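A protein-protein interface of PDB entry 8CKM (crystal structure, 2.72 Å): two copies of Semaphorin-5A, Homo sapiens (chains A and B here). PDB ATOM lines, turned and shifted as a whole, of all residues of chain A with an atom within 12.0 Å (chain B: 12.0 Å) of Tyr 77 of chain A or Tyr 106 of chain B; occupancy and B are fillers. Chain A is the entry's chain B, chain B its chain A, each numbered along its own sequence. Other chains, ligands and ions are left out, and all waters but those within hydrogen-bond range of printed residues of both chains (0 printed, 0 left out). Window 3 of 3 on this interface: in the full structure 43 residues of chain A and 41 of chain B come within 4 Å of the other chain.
The backbone carbonyl oxygen (O) of Thr 66 of chain A is in hydrogen-bond range of the backbone NH (N) of Gln 79 of chain A.
The backbone NH of Val 68 of chain A lies within hydrogen-bond range of the backbone carbonyl oxygen of Tyr 77 of chain A.
Thr 66 of chain A touches its own counterpart, Thr 66 of chain B.
Of the 18 pairs that touch across the chains among the printed residues, 1 has its exchanged pair printed and touching as well.
Among the printed residues, merely in contact across the chains: Trp 65 of chain A with Glu 103 of chain B (3.3 Å), Thr 66 of chain A with Thr 66 of chain B (3.5 Å), His 76 of chain A with Tyr 106 of chain B (3.7 Å), Tyr 77 of chain A with Arg 105 of chain B (3.5 Å), Tyr 77 of chain A with Tyr 106 of chain B (3.4 Å), Tyr 77 of chain A with Cys 107 of chain B (3.7 Å), Glu 78 of chain A with Glu 103 of chain B (3.9 Å), Glu 78 of chain A with Met 104 of chain B (3.3 Å), Gln 79 of chain A with Thr 66 of chain B (3.99 Å), Gln 79 of chain A with Ile 102 of chain B (3.8 Å), Gln 79 of chain A with Glu 103 of chain B (3.2 Å), Arg 80 of chain A with Ile 102 of chain B (3.4 Å) and Phe 81 of chain A with Ile 102 of chain B (3.7 Å).
Of chain B, only Arg 105 (3.5 Å), Tyr 106 (3.4 Å) and Cys 107 (3.7 Å) come within 4 Å of Tyr 77 of chain A.
No residue of chain B comes within 4 Å of Pro 67 of chain A.
Val 68 of chain A touches none of the printed residues of chain B.
Glu 78 of chain A touches just these residues of chain B: Glu 103 (3.9 Å), Met 104 (3.3 Å), Arg 105 (2.6 Å) and Cys 107 (3.6 Å).
Of chain A, only Glu 78 comes within 4 Å of Met 104 of chain B.
Of chain A, only Trp 65 (3.5 Å), Tyr 77 (3.5 Å) and Glu 78 (2.6 Å) come within 4 Å of Arg 105 of chain B.
Printed residues of chain B within 4 Å of Thr 66 of chain A: Thr 66 (3.5 Å).
Of the printed residues of chain A, Ile 102 of chain B touches Gln 79 (3.8 Å), Arg 80 (3.4 Å) and Phe 81 (3.7 Å).
Of the printed residues of chain B, Gln 79 of chain A touches Thr 66 (3.99 Å), Ile 102 (3.8 Å) and Glu 103 (3.2 Å).
Val 68 of chain B touches none of the printed residues of chain A.
Trp 65 of chain B touches none of the printed residues of chain A.
The nearest residue of chain B that does not touch Tyr 77 of chain A is Met 104 of chain B (4.1 Å).
The nearest residue of chain A that does not touch Tyr 106 of chain B is Glu 78 of chain A (4.5 Å).
The nearest printed residue of chain B that does not touch Thr 66 of chain A is Pro 67 of chain B (4.4 Å).
Of the 10 printed residues of chain B, 7 touch a printed residue of chain A.
Printed residues of chain B that touch a printed residue of chain A: Thr 66, Ile 102, Glu 103, Met 104, Arg 105, Tyr 106 and Cys 107.
Hydrophobic or aromatic side chains of chain B within 4 Å of the printed part of chain A: Ile 102, Met 104 and Tyr 106.
Of the 12 printed residues of chain A, 8 touch a printed residue of chain B.
Printed residues of chain A that touch a printed residue of chain B: Trp 65, Thr 66, His 76, Tyr 77, Glu 78, Gln 79, Arg 80 and Phe 81.
Hydrophobic or aromatic side chains of chain A that line the printed part of chain B: Trp 65, Tyr 77 and Phe 81.
Among the printed residues, Asp or Glu carboxylates within 4 Å of a Lys or Arg side-chain nitrogen of the other chain: Glu 78 of chain A with Arg 105 of chain B (2.6 Å) and Arg 80 of chain A with Glu 103 of chain B (2.7 Å).
OE1 of Glu 103 of chain B is in salt-bridge range of NH2 of Arg 80 of chain A (2.7 Å).
OE2 of Glu 78 of chain A is in salt-bridge range of NE of Arg 105 of chain B.
O of His 76 of chain A lies within hydrogen-bond range of N of Cys 107 of chain B.
The side-chain sulfur of Cys 107 of chain B lies close to the backbone NH of Glu 78 of chain A (3.6 Å).
NE1 of Trp 65 of chain A sits close to NH2 of Arg 105 of chain B (3.5 Å).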
ATOM      1  N   PRO A  64     -10.682  36.120 -10.692  1.00  0.00           N
ATOM      2  CA  PRO A  64      -9.885  34.913 -10.938  1.00  0.00           C
ATOM      3  C   PRO A  64     -10.581  33.667 -10.407  1.00  0.00           C
ATOM      4  O   PRO A  64     -11.291  33.706  -9.399  1.00  0.00           O
ATOM      5  CB  PRO A  64      -8.578  35.190 -10.185  1.00  0.00           C
ATOM      6  CG  PRO A  64      -8.925  36.250  -9.190  1.00  0.00           C
ATOM      7  CD  PRO A  64      -9.952  37.096  -9.867  1.00  0.00           C
ATOM      8  N   TRP A  65     -10.384  32.558 -11.118  1.00  0.00           N
ATOM      9  CA  TRP A  65     -10.954  31.283 -10.704  1.00  0.00           C
ATOM     10  C   TRP A  65     -10.411  30.876  -9.338  1.00  0.00           C
ATOM     11  O   TRP A  65      -9.202  30.919  -9.100  1.00  0.00           O
ATOM     12  CB  TRP A  65     -10.634  30.199 -11.734  1.00  0.00           C
ATOM     13  CG  TRP A  65     -11.337  30.349 -13.051  1.00  0.00           C
ATOM     14  CD1 TRP A  65     -10.870  30.987 -14.163  1.00  0.00           C
ATOM     15  CD2 TRP A  65     -12.625  29.826 -13.399  1.00  0.00           C
ATOM     16  NE1 TRP A  65     -11.790  30.899 -15.181  1.00  0.00           N
ATOM     17  CE2 TRP A  65     -12.876  30.191 -14.737  1.00  0.00           C
ATOM     18  CE3 TRP A  65     -13.591  29.087 -12.709  1.00  0.00           C
ATOM     19  CZ2 TRP A  65     -14.056  29.844 -15.398  1.00  0.00           C
ATOM     20  CZ3 TRP A  65     -14.763  28.745 -13.366  1.00  0.00           C
ATOM     21  CH2 TRP A  65     -14.983  29.122 -14.695  1.00  0.00           C
ATOM     22  N   THR A  66     -11.313  30.478  -8.442  1.00  0.00           N
ATOM     23  CA  THR A  66     -10.944  30.103  -7.088  1.00  0.00           C
ATOM     24  C   THR A  66     -11.635  28.797  -6.702  1.00  0.00           C
ATOM     25  O   THR A  66     -12.788  28.575  -7.083  1.00  0.00           O
ATOM     26  CB  THR A  66     -11.329  31.200  -6.083  1.00  0.00           C
ATOM     27  OG1 THR A  66     -12.723  31.505  -6.215  1.00  0.00           O
ATOM     28  CG2 THR A  66     -10.513  32.459  -6.323  1.00  0.00           C
ATOM     29  N   PRO A  67     -10.964  27.936  -5.943  1.00  0.00           N
ATOM     30  CA  PRO A  67     -11.595  26.678  -5.525  1.00  0.00           C
ATOM     31  C   PRO A  67     -12.742  26.921  -4.558  1.00  0.00           C
ATOM     32  O   PRO A  67     -12.850  27.969  -3.920  1.00  0.00           O
ATOM     33  CB  PRO A  67     -10.452  25.916  -4.848  1.00  0.00           C
ATOM     34  CG  PRO A  67      -9.515  26.982  -4.392  1.00  0.00           C
ATOM     35  CD  PRO A  67      -9.586  28.054  -5.440  1.00  0.00           C
ATOM     36  N   VAL A  68     -13.615  25.925  -4.469  1.00  0.00           N
ATOM     37  CA  VAL A  68     -14.791  25.984  -3.609  1.00  0.00           C
ATOM     38  C   VAL A  68     -14.537  25.304  -2.271  1.00  0.00           C
ATOM     39  O   VAL A  68     -14.800  25.878  -1.214  1.00  0.00           O
ATOM     40  CB  VAL A  68     -16.009  25.367  -4.330  1.00  0.00           C
ATOM     41  CG1 VAL A  68     -17.234  25.394  -3.428  1.00  0.00           C
ATOM     42  CG2 VAL A  68     -16.285  26.100  -5.633  1.00  0.00           C
ATOM     43  N   ASN A  69     -14.023  24.080  -2.296  1.00  0.00           N
ATOM     44  CA  ASN A  69     -13.761  23.337  -1.068  1.00  0.00           C
ATOM     45  C   ASN A  69     -12.271  23.050  -0.907  1.00  0.00           C
ATOM     46  O   ASN A  69     -11.791  21.978  -1.275  1.00  0.00           O
ATOM     47  CB  ASN A  69     -14.554  22.028  -1.055  1.00  0.00           C
ATOM     48  CG  ASN A  69     -16.054  22.254  -1.089  1.00  0.00           C
ATOM     49  OD1 ASN A  69     -16.561  23.216  -0.512  1.00  0.00           O
ATOM     50  ND2 ASN A  69     -16.771  21.369  -1.772  1.00  0.00           N
ATOM     51  N   HIS A  76     -13.671  18.573  -6.436  1.00  0.00           N
ATOM     52  CA  HIS A  76     -13.090  19.909  -6.435  1.00  0.00           C
ATOM     53  C   HIS A  76     -13.602  20.727  -7.618  1.00  0.00           C
ATOM     54  O   HIS A  76     -13.359  20.382  -8.778  1.00  0.00           O
ATOM     55  CB  HIS A  76     -11.566  19.833  -6.474  1.00  0.00           C
ATOM     56  N   TYR A  77     -14.296  21.822  -7.316  1.00  0.00           N
ATOM     57  CA  TYR A  77     -14.809  22.741  -8.321  1.00  0.00           C
ATOM     58  C   TYR A  77     -14.167  24.107  -8.121  1.00  0.00           C
ATOM     59  O   TYR A  77     -13.759  24.462  -7.010  1.00  0.00           O
ATOM     60  CB  TYR A  77     -16.341  22.873  -8.248  1.00  0.00           C
ATOM     61  CG  TYR A  77     -17.122  21.671  -8.760  1.00  0.00           C
ATOM     62  CD1 TYR A  77     -16.479  20.491  -9.113  1.00  0.00           C
ATOM     63  CD2 TYR A  77     -18.505  21.726  -8.914  1.00  0.00           C
ATOM     64  CE1 TYR A  77     -17.188  19.392  -9.584  1.00  0.00           C
ATOM     65  CE2 TYR A  77     -19.223  20.633  -9.392  1.00  0.00           C
ATOM     66  CZ  TYR A  77     -18.559  19.471  -9.726  1.00  0.00           C
ATOM     67  OH  TYR A  77     -19.259  18.381 -10.201  1.00  0.00           O
ATOM     68  N   GLU A  78     -14.069  24.867  -9.208  1.00  0.00           N
ATOM     69  CA  GLU A  78     -13.554  26.227  -9.162  1.00  0.00           C
ATOM     70  C   GLU A  78     -14.611  27.193  -9.678  1.00  0.00           C
ATOM     71  O   GLU A  78     -15.347  26.884 -10.621  1.00  0.00           O
ATOM     72  CB  GLU A  78     -12.256  26.362  -9.968  1.00  0.00           C
ATOM     73  CG  GLU A  78     -12.323  25.845 -11.391  1.00  0.00           C
ATOM     74  CD  GLU A  78     -11.004  26.002 -12.131  1.00  0.00           C
ATOM     75  OE1 GLU A  78     -10.037  26.512 -11.528  1.00  0.00           O
ATOM     76  OE2 GLU A  78     -10.936  25.616 -13.317  1.00  0.00           O
ATOM     77  N   GLN A  79     -14.682  28.364  -9.046  1.00  0.00           N
ATOM     78  CA  GLN A  79     -15.728  29.339  -9.318  1.00  0.00           C
ATOM     79  C   GLN A  79     -15.122  30.728  -9.488  1.00  0.00           C
ATOM     80  O   GLN A  79     -13.981  30.988  -9.093  1.00  0.00           O
ATOM     81  CB  GLN A  79     -16.774  29.364  -8.195  1.00  0.00           C
ATOM     82  CG  GLN A  79     -16.190  29.759  -6.848  1.00  0.00           C
ATOM     83  CD  GLN A  79     -17.215  29.774  -5.730  1.00  0.00           C
ATOM     84  OE1 GLN A  79     -18.423  29.845  -5.973  1.00  0.00           O
ATOM     85  NE2 GLN A  79     -16.737  29.705  -4.492  1.00  0.00           N
ATOM     86  N   ARG A  80     -15.911  31.618 -10.088  1.00  0.00           N
ATOM     87  CA  ARG A  80     -15.534  33.015 -10.256  1.00  0.00           C
ATOM     88  C   ARG A  80     -16.801  33.847 -10.401  1.00  0.00           C
ATOM     89  O   ARG A  80     -17.886  33.319 -10.654  1.00  0.00           O
ATOM     90  CB  ARG A  80     -14.600  33.215 -11.455  1.00  0.00           C
ATOM     91  CG  ARG A  80     -15.191  32.846 -12.801  1.00  0.00           C
ATOM     92  CD  ARG A  80     -14.253  33.262 -13.930  1.00  0.00           C
ATOM     93  NE  ARG A  80     -14.821  32.989 -15.245  1.00  0.00           N
ATOM     94  CZ  ARG A  80     -14.215  33.256 -16.395  1.00  0.00           C
ATOM     95  NH1 ARG A  80     -13.017  33.815 -16.433  1.00  0.00           N
ATOM     96  NH2 ARG A  80     -14.828  32.953 -17.537  1.00  0.00           N
ATOM     97  N   PHE A  81     -16.654  35.163 -10.229  1.00  0.00           N
ATOM     98  CA  PHE A  81     -17.800  36.047 -10.068  1.00  0.00           C
ATOM     99  C   PHE A  81     -17.649  37.311 -10.905  1.00  0.00           C
ATOM    100  O   PHE A  81     -16.538  37.751 -11.210  1.00  0.00           O
ATOM    101  CB  PHE A  81     -18.002  36.438  -8.593  1.00  0.00           C
ATOM    102  CG  PHE A  81     -17.996  35.273  -7.643  1.00  0.00           C
ATOM    103  CD1 PHE A  81     -16.799  34.746  -7.183  1.00  0.00           C
ATOM    104  CD2 PHE A  81     -19.182  34.713  -7.200  1.00  0.00           C
ATOM    105  CE1 PHE A  81     -16.782  33.675  -6.316  1.00  0.00           C
ATOM    106  CE2 PHE A  81     -19.172  33.643  -6.326  1.00  0.00           C
ATOM    107  CZ  PHE A  81     -17.969  33.124  -5.882  1.00  0.00           C
ATOM    108  N   TRP B  65     -15.959  35.406   0.324  1.00  0.00           N
ATOM    109  CA  TRP B  65     -14.554  35.174   0.627  1.00  0.00           C
ATOM    110  C   TRP B  65     -14.119  33.812   0.099  1.00  0.00           C
ATOM    111  O   TRP B  65     -14.778  32.799   0.350  1.00  0.00           O
ATOM    112  CB  TRP B  65     -14.312  35.260   2.135  1.00  0.00           C
ATOM    113  CG  TRP B  65     -14.430  36.645   2.705  1.00  0.00           C
ATOM    114  CD1 TRP B  65     -15.546  37.222   3.240  1.00  0.00           C
ATOM    115  CD2 TRP B  65     -13.387  37.621   2.811  1.00  0.00           C
ATOM    116  NE1 TRP B  65     -15.264  38.497   3.667  1.00  0.00           N
ATOM    117  CE2 TRP B  65     -13.943  38.764   3.417  1.00  0.00           C
ATOM    118  CE3 TRP B  65     -12.036  37.639   2.452  1.00  0.00           C
ATOM    119  CZ2 TRP B  65     -13.199  39.914   3.667  1.00  0.00           C
ATOM    120  CZ3 TRP B  65     -11.299  38.780   2.701  1.00  0.00           C
ATOM    121  CH2 TRP B  65     -11.882  39.902   3.303  1.00  0.00           C
ATOM    122  N   THR B  66     -13.006  33.789  -0.634  1.00  0.00           N
ATOM    123  CA  THR B  66     -12.440  32.564  -1.180  1.00  0.00           C
ATOM    124  C   THR B  66     -10.963  32.482  -0.849  1.00  0.00           C
ATOM    125  O   THR B  66     -10.259  33.501  -0.869  1.00  0.00           O
ATOM    126  CB  THR B  66     -12.627  32.491  -2.705  1.00  0.00           C
ATOM    127  OG1 THR B  66     -12.101  33.678  -3.313  1.00  0.00           O
ATOM    128  CG2 THR B  66     -14.097  32.341  -3.066  1.00  0.00           C
ATOM    129  N   PRO B  67     -10.447  31.290  -0.553  1.00  0.00           N
ATOM    130  CA  PRO B  67      -9.029  31.156  -0.216  1.00  0.00           C
ATOM    131  C   PRO B  67      -8.134  31.423  -1.417  1.00  0.00           C
ATOM    132  O   PRO B  67      -8.542  31.309  -2.575  1.00  0.00           O
ATOM    133  CB  PRO B  67      -8.908  29.703   0.254  1.00  0.00           C
ATOM    134  CG  PRO B  67     -10.032  29.001  -0.431  1.00  0.00           C
ATOM    135  CD  PRO B  67     -11.153  29.996  -0.500  1.00  0.00           C
ATOM    136  N   VAL B  68      -6.894  31.796  -1.120  1.00  0.00           N
ATOM    137  CA  VAL B  68      -5.898  32.033  -2.157  1.00  0.00           C
ATOM    138  C   VAL B  68      -4.976  30.825  -2.280  1.00  0.00           C
ATOM    139  O   VAL B  68      -4.764  30.302  -3.373  1.00  0.00           O
ATOM    140  CB  VAL B  68      -5.086  33.306  -1.874  1.00  0.00           C
ATOM    141  CG1 VAL B  68      -4.059  33.532  -2.972  1.00  0.00           C
ATOM    142  CG2 VAL B  68      -6.008  34.505  -1.748  1.00  0.00           C
ATOM    143  N   ILE B 102     -22.225  33.743 -11.017  1.00  0.00           N
ATOM    144  CA  ILE B 102     -21.250  32.733 -10.623  1.00  0.00           C
ATOM    145  C   ILE B 102     -21.035  31.790 -11.797  1.00  0.00           C
ATOM    146  O   ILE B 102     -22.001  31.277 -12.370  1.00  0.00           O
ATOM    147  CB  ILE B 102     -21.715  31.958  -9.381  1.00  0.00           C
ATOM    148  CG1 ILE B 102     -22.247  32.924  -8.315  1.00  0.00           C
ATOM    149  CG2 ILE B 102     -20.576  31.123  -8.816  1.00  0.00           C
ATOM    150  CD1 ILE B 102     -22.868  32.225  -7.123  1.00  0.00           C
ATOM    151  N   GLU B 103     -19.775  31.574 -12.163  1.00  0.00           N
ATOM    152  CA  GLU B 103     -19.401  30.611 -13.191  1.00  0.00           C
ATOM    153  C   GLU B 103     -18.525  29.546 -12.550  1.00  0.00           C
ATOM    154  O   GLU B 103     -17.513  29.871 -11.919  1.00  0.00           O
ATOM    155  CB  GLU B 103     -18.670  31.281 -14.356  1.00  0.00           C
ATOM    156  CG  GLU B 103     -18.344  30.336 -15.509  1.00  0.00           C
ATOM    157  CD  GLU B 103     -17.600  31.032 -16.635  1.00  0.00           C
ATOM    158  OE1 GLU B 103     -17.191  32.198 -16.449  1.00  0.00           O
ATOM    159  OE2 GLU B 103     -17.421  30.417 -17.710  1.00  0.00           O
ATOM    160  N   MET B 104     -18.908  28.280 -12.722  1.00  0.00           N
ATOM    161  CA  MET B 104     -18.251  27.162 -12.061  1.00  0.00           C
ATOM    162  C   MET B 104     -17.808  26.124 -13.078  1.00  0.00           C
ATOM    163  O   MET B 104     -18.507  25.876 -14.062  1.00  0.00           O
ATOM    164  CB  MET B 104     -19.192  26.507 -11.037  1.00  0.00           C
ATOM    165  CG  MET B 104     -19.871  27.474 -10.085  1.00  0.00           C
ATOM    166  SD  MET B 104     -20.998  26.647  -8.945  1.00  0.00           S
ATOM    167  CE  MET B 104     -19.873  25.544  -8.091  1.00  0.00           C
ATOM    168  N   ARG B 105     -16.646  25.523 -12.836  1.00  0.00           N
ATOM    169  CA  ARG B 105     -16.201  24.376 -13.611  1.00  0.00           C
ATOM    170  C   ARG B 105     -15.434  23.442 -12.689  1.00  0.00           C
ATOM    171  O   ARG B 105     -14.970  23.836 -11.618  1.00  0.00           O
ATOM    172  CB  ARG B 105     -15.345  24.786 -14.811  1.00  0.00           C
ATOM    173  CG  ARG B 105     -14.062  25.491 -14.459  1.00  0.00           C
ATOM    174  CD  ARG B 105     -13.331  25.925 -15.711  1.00  0.00           C
ATOM    175  NE  ARG B 105     -12.122  26.685 -15.417  1.00  0.00           N
ATOM    176  CZ  ARG B 105     -11.323  27.199 -16.340  1.00  0.00           C
ATOM    177  NH1 ARG B 105     -11.578  27.053 -17.630  1.00  0.00           N
ATOM    178  NH2 ARG B 105     -10.243  27.876 -15.961  1.00  0.00           N
ATOM    179  N   TYR B 106     -15.311  22.193 -13.106  1.00  0.00           N
ATOM    180  CA  TYR B 106     -14.760  21.170 -12.234  1.00  0.00           C
ATOM    181  C   TYR B 106     -13.249  21.056 -12.394  1.00  0.00           C
ATOM    182  O   TYR B 106     -12.678  21.435 -13.420  1.00  0.00           O
ATOM    183  CB  TYR B 106     -15.421  19.817 -12.510  1.00  0.00           C
ATOM    184  N   CYS B 107     -12.610  20.539 -11.348  1.00  0.00           N
ATOM    185  CA  CYS B 107     -11.183  20.272 -11.314  1.00  0.00           C
ATOM    186  C   CYS B 107     -10.977  18.777 -11.094  1.00  0.00           C
ATOM    187  O   CYS B 107     -10.050  18.176 -11.625  1.00  0.00           O
ATOM    188  CB  CYS B 107     -10.508  21.083 -10.197  1.00  0.00           C
ATOM    189  SG  CYS B 107     -11.232  22.720  -9.931  1.00  0.00           S
